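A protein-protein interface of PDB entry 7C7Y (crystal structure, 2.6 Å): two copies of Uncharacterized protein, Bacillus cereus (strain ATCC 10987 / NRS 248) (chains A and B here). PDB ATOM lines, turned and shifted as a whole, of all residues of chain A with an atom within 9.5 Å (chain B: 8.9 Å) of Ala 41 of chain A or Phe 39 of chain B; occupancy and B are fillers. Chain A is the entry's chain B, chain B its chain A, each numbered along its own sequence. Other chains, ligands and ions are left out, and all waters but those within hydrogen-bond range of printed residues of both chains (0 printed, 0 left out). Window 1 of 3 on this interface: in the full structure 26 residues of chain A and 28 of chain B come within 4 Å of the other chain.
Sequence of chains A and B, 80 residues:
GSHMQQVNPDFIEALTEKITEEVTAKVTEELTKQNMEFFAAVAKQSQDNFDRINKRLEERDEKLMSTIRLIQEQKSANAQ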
ATOM      1  N   GLN A  34     -31.304 -18.506  -8.987  1.00  0.00           N
ATOM      2  CA  GLN A  34     -31.420 -19.735  -8.157  1.00  0.00           C
ATOM      3  C   GLN A  34     -30.243 -20.667  -8.439  1.00  0.00           C
ATOM      4  O   GLN A  34     -29.676 -21.212  -7.469  1.00  0.00           O
ATOM      5  CB  GLN A  34     -32.709 -20.478  -8.472  1.00  0.00           C
ATOM      6  CG  GLN A  34     -33.140 -21.430  -7.371  1.00  0.00           C
ATOM      7  CD  GLN A  34     -34.629 -21.673  -7.438  1.00  0.00           C
ATOM      8  OE1 GLN A  34     -35.440 -20.835  -7.047  1.00  0.00           O
ATOM      9  NE2 GLN A  34     -35.005 -22.834  -7.951  1.00  0.00           N
ATOM     10  N   ASN A  35     -29.891 -20.808  -9.719  1.00  0.00           N
ATOM     11  CA  ASN A  35     -28.822 -21.708 -10.230  1.00  0.00           C
ATOM     12  C   ASN A  35     -27.437 -21.273  -9.745  1.00  0.00           C
ATOM     13  O   ASN A  35     -26.645 -22.153  -9.371  1.00  0.00           O
ATOM     14  CB  ASN A  35     -28.811 -21.750 -11.757  1.00  0.00           C
ATOM     15  CG  ASN A  35     -29.765 -22.772 -12.328  1.00  0.00           C
ATOM     16  OD1 ASN A  35     -30.387 -23.557 -11.595  1.00  0.00           O
ATOM     17  ND2 ASN A  35     -29.863 -22.775 -13.645  1.00  0.00           N
ATOM     18  N   MET A  36     -27.126 -19.981  -9.819  1.00  0.00           N
ATOM     19  CA  MET A  36     -25.845 -19.425  -9.327  1.00  0.00           C
ATOM     20  C   MET A  36     -25.701 -19.796  -7.850  1.00  0.00           C
ATOM     21  O   MET A  36     -24.709 -20.445  -7.494  1.00  0.00           O
ATOM     22  CB  MET A  36     -25.841 -17.909  -9.513  1.00  0.00           C
ATOM     23  CG  MET A  36     -25.764 -17.472 -10.950  1.00  0.00           C
ATOM     24  SD  MET A  36     -25.183 -15.598 -11.038  1.00  0.00           S
ATOM     25  CE  MET A  36     -23.710 -15.460 -12.338  1.00  0.00           C
ATOM     26  N   GLU A  37     -26.675 -19.398  -7.029  1.00  0.00           N
ATOM     27  CA  GLU A  37     -26.737 -19.725  -5.580  1.00  0.00           C
ATOM     28  C   GLU A  37     -26.587 -21.239  -5.419  1.00  0.00           C
ATOM     29  O   GLU A  37     -25.843 -21.660  -4.540  1.00  0.00           O
ATOM     30  CB  GLU A  37     -28.055 -19.232  -4.976  1.00  0.00           C
ATOM     31  CG  GLU A  37     -28.207 -19.479  -3.480  1.00  0.00           C
ATOM     32  CD  GLU A  37     -29.643 -19.454  -2.970  1.00  0.00           C
ATOM     33  OE1 GLU A  37     -30.491 -18.789  -3.606  1.00  0.00           O
ATOM     34  OE2 GLU A  37     -29.915 -20.109  -1.933  1.00  0.00           O
ATOM     35  N   PHE A  38     -27.274 -22.022  -6.247  1.00  0.00           N
ATOM     36  CA  PHE A  38     -27.289 -23.509  -6.184  1.00  0.00           C
ATOM     37  C   PHE A  38     -25.941 -24.093  -6.643  1.00  0.00           C
ATOM     38  O   PHE A  38     -25.434 -24.989  -5.937  1.00  0.00           O
ATOM     39  CB  PHE A  38     -28.443 -24.071  -7.022  1.00  0.00           C
ATOM     40  CG  PHE A  38     -28.408 -25.565  -7.210  1.00  0.00           C
ATOM     41  CD1 PHE A  38     -28.448 -26.414  -6.115  1.00  0.00           C
ATOM     42  CD2 PHE A  38     -28.290 -26.124  -8.474  1.00  0.00           C
ATOM     43  CE1 PHE A  38     -28.403 -27.793  -6.284  1.00  0.00           C
ATOM     44  CE2 PHE A  38     -28.248 -27.498  -8.640  1.00  0.00           C
ATOM     45  CZ  PHE A  38     -28.308 -28.329  -7.548  1.00  0.00           C
ATOM     46  N   PHE A  39     -25.390 -23.644  -7.781  1.00  0.00           N
ATOM     47  CA  PHE A  39     -24.143 -24.200  -8.366  1.00  0.00           C
ATOM     48  C   PHE A  39     -22.996 -23.967  -7.381  1.00  0.00           C
ATOM     49  O   PHE A  39     -22.289 -24.933  -7.013  1.00  0.00           O
ATOM     50  CB  PHE A  39     -23.829 -23.593  -9.736  1.00  0.00           C
ATOM     51  CG  PHE A  39     -24.749 -23.987 -10.869  1.00  0.00           C
ATOM     52  CD1 PHE A  39     -25.574 -25.102 -10.786  1.00  0.00           C
ATOM     53  CD2 PHE A  39     -24.760 -23.254 -12.047  1.00  0.00           C
ATOM     54  CE1 PHE A  39     -26.425 -25.439 -11.830  1.00  0.00           C
ATOM     55  CE2 PHE A  39     -25.595 -23.606 -13.095  1.00  0.00           C
ATOM     56  CZ  PHE A  39     -26.428 -24.697 -12.985  1.00  0.00           C
ATOM     57  N   ALA A  40     -22.843 -22.717  -6.939  1.00  0.00           N
ATOM     58  CA  ALA A  40     -21.843 -22.300  -5.929  1.00  0.00           C
ATOM     59  C   ALA A  40     -21.779 -23.327  -4.784  1.00  0.00           C
ATOM     60  O   ALA A  40     -20.666 -23.719  -4.442  1.00  0.00           O
ATOM     61  CB  ALA A  40     -22.162 -20.915  -5.429  1.00  0.00           C
ATOM     62  N   ALA A  41     -22.919 -23.778  -4.243  1.00  0.00           N
ATOM     63  CA  ALA A  41     -23.005 -24.661  -3.047  1.00  0.00           C
ATOM     64  C   ALA A  41     -22.629 -26.107  -3.395  1.00  0.00           C
ATOM     65  O   ALA A  41     -22.078 -26.791  -2.526  1.00  0.00           O
ATOM     66  CB  ALA A  41     -24.381 -24.620  -2.437  1.00  0.00           C
ATOM     67  N   VAL A  42     -22.926 -26.567  -4.605  1.00  0.00           N
ATOM     68  CA  VAL A  42     -22.402 -27.872  -5.098  1.00  0.00           C
ATOM     69  C   VAL A  42     -20.862 -27.747  -5.159  1.00  0.00           C
ATOM     70  O   VAL A  42     -20.149 -28.577  -4.563  1.00  0.00           O
ATOM     71  CB  VAL A  42     -23.043 -28.267  -6.447  1.00  0.00           C
ATOM     72  CG1 VAL A  42     -22.671 -29.681  -6.846  1.00  0.00           C
ATOM     73  CG2 VAL A  42     -24.559 -28.143  -6.430  1.00  0.00           C
ATOM     74  N   ALA A  43     -20.364 -26.697  -5.805  1.00  0.00           N
ATOM     75  CA  ALA A  43     -18.927 -26.482  -6.083  1.00  0.00           C
ATOM     76  C   ALA A  43     -18.108 -26.349  -4.783  1.00  0.00           C
ATOM     77  O   ALA A  43     -16.950 -26.811  -4.799  1.00  0.00           O
ATOM     78  CB  ALA A  43     -18.780 -25.271  -6.969  1.00  0.00           C
ATOM     79  N   LYS A  44     -18.650 -25.743  -3.714  1.00  0.00           N
ATOM     80  CA  LYS A  44     -17.907 -25.507  -2.439  1.00  0.00           C
ATOM     81  C   LYS A  44     -17.872 -26.813  -1.640  1.00  0.00           C
ATOM     82  O   LYS A  44     -16.800 -27.164  -1.077  1.00  0.00           O
ATOM     83  CB  LYS A  44     -18.534 -24.418  -1.555  1.00  0.00           C
ATOM     84  CG  LYS A  44     -18.092 -24.453  -0.089  1.00  0.00           C
ATOM     85  CD  LYS A  44     -18.890 -23.603   0.898  1.00  0.00           C
ATOM     86  CE  LYS A  44     -18.736 -24.052   2.341  1.00  0.00           C
ATOM     87  NZ  LYS A  44     -17.317 -23.993   2.792  1.00  0.00           N
ATOM     88  N   GLN A  45     -19.028 -27.465  -1.540  1.00  0.00           N
ATOM     89  CA  GLN A  45     -19.163 -28.806  -0.927  1.00  0.00           C
ATOM     90  C   GLN A  45     -18.175 -29.747  -1.619  1.00  0.00           C
ATOM     91  O   GLN A  45     -17.487 -30.521  -0.917  1.00  0.00           O
ATOM     92  CB  GLN A  45     -20.604 -29.276  -1.074  1.00  0.00           C
ATOM     93  CG  GLN A  45     -20.803 -30.775  -0.961  1.00  0.00           C
ATOM     94  CD  GLN A  45     -21.890 -31.148  -1.933  1.00  0.00           C
ATOM     95  OE1 GLN A  45     -21.665 -31.251  -3.144  1.00  0.00           O
ATOM     96  NE2 GLN A  45     -23.092 -31.291  -1.402  1.00  0.00           N
ATOM     97  N   SER A  46     -18.108 -29.682  -2.947  1.00  0.00           N
ATOM     98  CA  SER A  46     -17.171 -30.500  -3.741  1.00  0.00           C
ATOM     99  C   SER A  46     -15.744 -30.214  -3.236  1.00  0.00           C
ATOM    100  O   SER A  46     -15.145 -31.154  -2.659  1.00  0.00           O
ATOM    101  CB  SER A  46     -17.359 -30.255  -5.216  1.00  0.00           C
ATOM    102  OG  SER A  46     -16.149 -30.473  -5.924  1.00  0.00           O
ATOM    103  N   GLN A  47     -15.242 -28.967  -3.342  1.00  0.00           N
ATOM    104  CA  GLN A  47     -13.837 -28.612  -2.966  1.00  0.00           C
ATOM    105  C   GLN A  47     -13.627 -28.842  -1.475  1.00  0.00           C
ATOM    106  O   GLN A  47     -12.531 -29.227  -1.116  1.00  0.00           O
ATOM    107  CB  GLN A  47     -13.452 -27.160  -3.247  1.00  0.00           C
ATOM    108  CG  GLN A  47     -12.713 -26.930  -4.560  1.00  0.00           C
ATOM    109  CD  GLN A  47     -11.284 -27.427  -4.582  1.00  0.00           C
ATOM    110  OE1 GLN A  47     -10.575 -27.409  -3.569  1.00  0.00           O
ATOM    111  NE2 GLN A  47     -10.838 -27.861  -5.759  1.00  0.00           N
ATOM    112  N   ASP A  48     -14.619 -28.590  -0.623  1.00  0.00           N
ATOM    113  CA  ASP A  48     -14.456 -28.865   0.831  1.00  0.00           C
ATOM    114  C   ASP A  48     -14.172 -30.358   1.003  1.00  0.00           C
ATOM    115  O   ASP A  48     -13.414 -30.702   1.903  1.00  0.00           O
ATOM    116  CB  ASP A  48     -15.670 -28.475   1.666  1.00  0.00           C
ATOM    117  CG  ASP A  48     -15.946 -26.986   1.729  1.00  0.00           C
ATOM    118  OD1 ASP A  48     -15.030 -26.204   1.431  1.00  0.00           O
ATOM    119  OD2 ASP A  48     -17.088 -26.625   2.087  1.00  0.00           O
ATOM    120  N   ASN A  49     -14.749 -31.207   0.153  1.00  0.00           N
ATOM    121  CA  ASN A  49     -14.577 -32.677   0.248  1.00  0.00           C
ATOM    122  C   ASN A  49     -13.171 -33.055  -0.236  1.00  0.00           C
ATOM    123  O   ASN A  49     -12.502 -33.808   0.474  1.00  0.00           O
ATOM    124  CB  ASN A  49     -15.671 -33.435  -0.500  1.00  0.00           C
ATOM    125  CG  ASN A  49     -15.852 -34.796   0.116  1.00  0.00           C
ATOM    126  OD1 ASN A  49     -16.044 -34.903   1.324  1.00  0.00           O
ATOM    127  ND2 ASN A  49     -15.733 -35.832  -0.690  1.00  0.00           N
ATOM    128  N   LEU B  31     -38.126 -25.450  -8.369  1.00  0.00           N
ATOM    129  CA  LEU B  31     -36.713 -25.732  -8.724  1.00  0.00           C
ATOM    130  C   LEU B  31     -35.847 -25.583  -7.467  1.00  0.00           C
ATOM    131  O   LEU B  31     -34.743 -26.161  -7.463  1.00  0.00           O
ATOM    132  CB  LEU B  31     -36.254 -24.818  -9.867  1.00  0.00           C
ATOM    133  CG  LEU B  31     -35.162 -25.410 -10.771  1.00  0.00           C
ATOM    134  CD1 LEU B  31     -35.537 -25.263 -12.235  1.00  0.00           C
ATOM    135  CD2 LEU B  31     -33.781 -24.801 -10.508  1.00  0.00           C
ATOM    136  N   THR B  32     -36.339 -24.857  -6.448  1.00  0.00           N
ATOM    137  CA  THR B  32     -35.686 -24.671  -5.123  1.00  0.00           C
ATOM    138  C   THR B  32     -35.758 -25.982  -4.344  1.00  0.00           C
ATOM    139  O   THR B  32     -34.675 -26.524  -4.033  1.00  0.00           O
ATOM    140  CB  THR B  32     -36.333 -23.557  -4.285  1.00  0.00           C
ATOM    141  OG1 THR B  32     -35.884 -22.293  -4.777  1.00  0.00           O
ATOM    142  CG2 THR B  32     -36.001 -23.641  -2.808  1.00  0.00           C
ATOM    143  N   LYS B  33     -36.979 -26.450  -4.045  1.00  0.00           N
ATOM    144  CA  LYS B  33     -37.234 -27.726  -3.318  1.00  0.00           C
ATOM    145  C   LYS B  33     -36.459 -28.846  -4.010  1.00  0.00           C
ATOM    146  O   LYS B  33     -35.875 -29.657  -3.271  1.00  0.00           O
ATOM    147  CB  LYS B  33     -38.722 -28.079  -3.236  1.00  0.00           C
ATOM    148  CG  LYS B  33     -39.602 -27.086  -2.477  1.00  0.00           C
ATOM    149  CD  LYS B  33     -39.069 -26.621  -1.115  1.00  0.00           C
ATOM    150  CE  LYS B  33     -39.905 -25.533  -0.460  1.00  0.00           C
ATOM    151  NZ  LYS B  33     -39.913 -24.269  -1.244  1.00  0.00           N
ATOM    152  N   GLN B  34     -36.415 -28.842  -5.351  1.00  0.00           N
ATOM    153  CA  GLN B  34     -35.646 -29.818  -6.180  1.00  0.00           C
ATOM    154  C   GLN B  34     -34.152 -29.732  -5.846  1.00  0.00           C
ATOM    155  O   GLN B  34     -33.578 -30.767  -5.462  1.00  0.00           O
ATOM    156  CB  GLN B  34     -35.851 -29.601  -7.684  1.00  0.00           C
ATOM    157  CG  GLN B  34     -36.684 -30.694  -8.352  1.00  0.00           C
ATOM    158  CD  GLN B  34     -36.793 -30.578  -9.858  1.00  0.00           C
ATOM    159  OE1 GLN B  34     -35.795 -30.517 -10.579  1.00  0.00           O
ATOM    160  NE2 GLN B  34     -38.023 -30.586 -10.351  1.00  0.00           N
ATOM    161  N   ASN B  35     -33.553 -28.550  -6.012  1.00  0.00           N
ATOM    162  CA  ASN B  35     -32.126 -28.251  -5.710  1.00  0.00           C
ATOM    163  C   ASN B  35     -31.782 -28.583  -4.238  1.00  0.00           C
ATOM    164  O   ASN B  35     -30.623 -28.964  -3.994  1.00  0.00           O
ATOM    165  CB  ASN B  35     -31.805 -26.789  -6.028  1.00  0.00           C
ATOM    166  CG  ASN B  35     -31.835 -26.457  -7.507  1.00  0.00           C
ATOM    167  OD1 ASN B  35     -31.916 -27.341  -8.348  1.00  0.00           O
ATOM    168  ND2 ASN B  35     -31.765 -25.175  -7.833  1.00  0.00           N
ATOM    169  N   MET B  36     -32.732 -28.440  -3.299  1.00  0.00           N
ATOM    170  CA  MET B  36     -32.583 -28.791  -1.854  1.00  0.00           C
ATOM    171  C   MET B  36     -32.324 -30.295  -1.704  1.00  0.00           C
ATOM    172  O   MET B  36     -31.370 -30.652  -1.011  1.00  0.00           O
ATOM    173  CB  MET B  36     -33.837 -28.429  -1.046  1.00  0.00           C
ATOM    174  CG  MET B  36     -34.015 -26.952  -0.757  1.00  0.00           C
ATOM    175  SD  MET B  36     -32.655 -26.285   0.490  1.00  0.00           S
ATOM    176  CE  MET B  36     -31.000 -25.885  -0.503  1.00  0.00           C
ATOM    177  N   GLU B  37     -33.186 -31.134  -2.285  1.00  0.00           N
ATOM    178  CA  GLU B  37     -33.033 -32.614  -2.349  1.00  0.00           C
ATOM    179  C   GLU B  37     -31.634 -32.956  -2.871  1.00  0.00           C
ATOM    180  O   GLU B  37     -30.878 -33.629  -2.155  1.00  0.00           O
ATOM    181  CB  GLU B  37     -34.069 -33.253  -3.285  1.00  0.00           C
ATOM    182  CG  GLU B  37     -35.286 -33.820  -2.580  1.00  0.00           C
ATOM    183  CD  GLU B  37     -36.153 -32.789  -1.877  1.00  0.00           C
ATOM    184  OE1 GLU B  37     -35.639 -32.085  -0.977  1.00  0.00           O
ATOM    185  OE2 GLU B  37     -37.341 -32.686  -2.234  1.00  0.00           O
ATOM    186  N   PHE B  38     -31.312 -32.516  -4.086  1.00  0.00           N
ATOM    187  CA  PHE B  38     -30.046 -32.871  -4.767  1.00  0.00           C
ATOM    188  C   PHE B  38     -28.875 -32.460  -3.871  1.00  0.00           C
ATOM    189  O   PHE B  38     -28.021 -33.316  -3.606  1.00  0.00           O
ATOM    190  CB  PHE B  38     -29.927 -32.218  -6.149  1.00  0.00           C
ATOM    191  CG  PHE B  38     -28.635 -32.563  -6.854  1.00  0.00           C
ATOM    192  CD1 PHE B  38     -28.402 -33.855  -7.312  1.00  0.00           C
ATOM    193  CD2 PHE B  38     -27.622 -31.624  -6.988  1.00  0.00           C
ATOM    194  CE1 PHE B  38     -27.203 -34.180  -7.932  1.00  0.00           C
ATOM    195  CE2 PHE B  38     -26.425 -31.951  -7.605  1.00  0.00           C
ATOM    196  CZ  PHE B  38     -26.220 -33.227  -8.085  1.00  0.00           C
ATOM    197  N   PHE B  39     -28.836 -31.197  -3.428  1.00  0.00           N
ATOM    198  CA  PHE B  39     -27.787 -30.709  -2.500  1.00  0.00           C
ATOM    199  C   PHE B  39     -27.648 -31.714  -1.355  1.00  0.00           C
ATOM    200  O   PHE B  39     -26.555 -32.274  -1.173  1.00  0.00           O
ATOM    201  CB  PHE B  39     -28.080 -29.319  -1.934  1.00  0.00           C
ATOM    202  CG  PHE B  39     -26.933 -28.784  -1.114  1.00  0.00           C
ATOM    203  CD1 PHE B  39     -25.803 -28.287  -1.737  1.00  0.00           C
ATOM    204  CD2 PHE B  39     -26.951 -28.846   0.274  1.00  0.00           C
ATOM    205  CE1 PHE B  39     -24.729 -27.830  -0.988  1.00  0.00           C
ATOM    206  CE2 PHE B  39     -25.874 -28.386   1.018  1.00  0.00           C
ATOM    207  CZ  PHE B  39     -24.763 -27.880   0.387  1.00  0.00           C
ATOM    208  N   ALA B  40     -28.751 -31.953  -0.638  1.00  0.00           N
ATOM    209  CA  ALA B  40     -28.816 -32.824   0.555  1.00  0.00           C
ATOM    210  C   ALA B  40     -28.296 -34.217   0.199  1.00  0.00           C
ATOM    211  O   ALA B  40     -27.653 -34.827   1.046  1.00  0.00           O
ATOM    212  CB  ALA B  40     -30.228 -32.874   1.083  1.00  0.00           C
ATOM    213  N   ALA B  41     -28.559 -34.692  -1.015  1.00  0.00           N
ATOM    214  CA  ALA B  41     -28.189 -36.047  -1.483  1.00  0.00           C
ATOM    215  C   ALA B  41     -26.709 -36.102  -1.870  1.00  0.00           C
ATOM    216  O   ALA B  41     -26.120 -37.166  -1.669  1.00  0.00           O
ATOM    217  CB  ALA B  41     -29.065 -36.451  -2.639  1.00  0.00           C
ATOM    218  N   VAL B  42     -26.141 -35.028  -2.436  1.00  0.00           N
ATOM    219  CA  VAL B  42     -24.710 -34.997  -2.871  1.00  0.00           C
ATOM    220  C   VAL B  42     -23.855 -34.906  -1.606  1.00  0.00           C
ATOM    221  O   VAL B  42     -22.743 -35.451  -1.623  1.00  0.00           O
ATOM    222  CB  VAL B  42     -24.383 -33.850  -3.852  1.00  0.00           C
ATOM    223  CG1 VAL B  42     -22.898 -33.767  -4.181  1.00  0.00           C
ATOM    224  CG2 VAL B  42     -25.161 -33.983  -5.144  1.00  0.00           C
ATOM    225  N   ALA B  43     -24.368 -34.252  -0.559  1.00  0.00           N
ATOM    226  CA  ALA B  43     -23.707 -34.152   0.759  1.00  0.00           C
ATOM    227  C   ALA B  43     -23.596 -35.560   1.343  1.00  0.00           C
ATOM    228  O   ALA B  43     -22.467 -35.950   1.674  1.00  0.00           O
ATOM    229  CB  ALA B  43     -24.458 -33.228   1.684  1.00  0.00           C
ATOM    230  N   LYS B  44     -24.709 -36.303   1.427  1.00  0.00           N
ATOM    231  CA  LYS B  44     -24.719 -37.650   2.061  1.00  0.00           C
ATOM    232  C   LYS B  44     -23.785 -38.559   1.259  1.00  0.00           C
ATOM    233  O   LYS B  44     -22.927 -39.194   1.882  1.00  0.00           O
ATOM    234  CB  LYS B  44     -26.117 -38.266   2.179  1.00  0.00           C
ATOM    235  CG  LYS B  44     -26.147 -39.559   2.992  1.00  0.00           C
ATOM    236  CD  LYS B  44     -27.309 -40.483   2.700  1.00  0.00           C
ATOM    237  CE  LYS B  44     -27.125 -41.843   3.341  1.00  0.00           C
ATOM    238  NZ  LYS B  44     -28.404 -42.584   3.463  1.00  0.00           N
ATOM    239  N   GLN B  45     -23.908 -38.562  -0.066  1.00  0.00           N
ATOM    240  CA  GLN B  45     -22.967 -39.279  -0.978  1.00  0.00           C
ATOM    241  C   GLN B  45     -21.505 -38.883  -0.683  1.00  0.00           C
ATOM    242  O   GLN B  45     -20.660 -39.775  -0.607  1.00  0.00           O
ATOM    243  CB  GLN B  45     -23.333 -38.997  -2.440  1.00  0.00           C
ATOM    244  CG  GLN B  45     -22.290 -39.478  -3.439  1.00  0.00           C
ATOM    245  CD  GLN B  45     -22.153 -38.506  -4.584  1.00  0.00           C
ATOM    246  OE1 GLN B  45     -22.885 -38.594  -5.575  1.00  0.00           O
ATOM    247  NE2 GLN B  45     -21.236 -37.553  -4.437  1.00  0.00           N
ATOM    248  N   SER B  46     -21.214 -37.587  -0.547  1.00  0.00           N
ATOM    249  CA  SER B  46     -19.862 -37.006  -0.307  1.00  0.00           C
ATOM    250  C   SER B  46     -19.296 -37.556   1.012  1.00  0.00           C
ATOM    251  O   SER B  46     -18.128 -37.978   1.031  1.00  0.00           O
ATOM    252  CB  SER B  46     -19.933 -35.480  -0.296  1.00  0.00           C
ATOM    253  OG  SER B  46     -18.728 -34.882  -0.750  1.00  0.00           O
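The backbone carbonyl oxygen (O) of Leu 31 of chain B lies close to the side-chain amide nitrogen (ND2) of Asn 35 of chain B.
The side-chain amide oxygen (OE1) of Gln 45 of chain A sits close to the backbone carbonyl oxygen (O) of Val 42 of chain A, 3.4 Å away.
Phe 38 of chain A touches Asn 35 of chain B, but with the chains exchanged Asn 35 of chain A does not touch Phe 38 of chain B (9.7 Å).
Ala 41 of chain A touches Phe 39 of chain B, but with the chains exchanged Phe 39 of chain A does not touch Ala 41 of chain B (13.1 Å).
Gln 45 of chain A touches Val 42 of chain B, but with the chains exchanged Val 42 of chain A does not touch Gln 45 of chain B (8.4 Å).
Gln 45 of chain A touches Ala 43 of chain B, but with the chains exchanged Ala 43 of chain A does not touch Gln 45 of chain B (11.0 Å).
Positions printed for both chains: 34, 35, 36, 37, 38, 39, 40, 41, 42, 43, 44, 45 and 46.
Of the 11 pairs that touch across the chains among the printed residues, 1 has its exchanged pair printed and touching as well.
Hydrophobic or aromatic side chains of chain A that line the printed part of chain B: Phe 38 and Ala 41.
Along chain A the printed residues that touch a printed residue of chain B span positions 34 to 49.
Hydrophobic or aromatic side chains of chain B that line the printed part of chain A: Leu 31, Phe 38, Phe 39, Val 42 and Ala 43.
Among the printed residues, 11 pairs touch across the chains.
Among the printed residues, no Asp or Glu carboxylate lies within 4 Å of a Lys or Arg side-chain nitrogen of the other chain.
Asn 35 of chain B touches Gln 34 of chain A.
Leu 31 of chain B touches Asn 35 of chain A (CD2 to OD1, 3.8 Å).
CD1 of Phe 38 of chain A touches CB of Asn 35 of chain B (3.4 Å).
CZ of Phe 38 of chain A touches CD2 of Phe 38 of chain B (3.4 Å).
Ala 41 of chain A touches Phe 39 of chain B.
Gln 45 of chain A touches Phe 39 of chain B.
Gln 45 of chain A touches Val 42 of chain B.
The backbone carbonyl oxygen of Leu 31 of chain B lies close to the side-chain amide nitrogen of Gln 34 of chain A, at 3.4 Å.
N of Ala 43 of chain B sits close to NE2 of Gln 45 of chain A (3.3 Å).
The side-chain amide oxygen (OE1) of Gln 34 of chain A is in hydrogen-bond range of the side-chain hydroxyl (OG1) of Thr 32 of chain B.
OG of Ser 46 of chain B lies close to ND2 of Asn 49 of chain A, at 3.1 Å.
Of the printed residues of chain B, Gln 34 of chain A touches Leu 31 (2.9 Å), Thr 32 (2.7 Å) and Asn 35 (3.999 Å).
Met 36 of chain A touches none of the printed residues of chain B.
Glu 37 of chain A touches none of the printed residues of chain B.
Ala 41 of chain A touches one residue of chain B.
Printed residues of chain B within 4 Å of Gln 45 of chain A: Phe 39 (3.6 Å), Val 42 (3.0 Å) and Ala 43 (3.3 Å).
No residue of chain A comes within 4 Å of Ala 40 of chain B.
Of chain A, only Gln 45 (3.0 Å) comes within 4 Å of Val 42 of chain B.
The nearest residue of chain B that does not touch Ala 41 of chain A is Met 36 of chain B (7.0 Å).
The nearest printed residue of chain A that does not touch Asn 35 of chain B is Asn 35 of chain A (4.3 Å).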
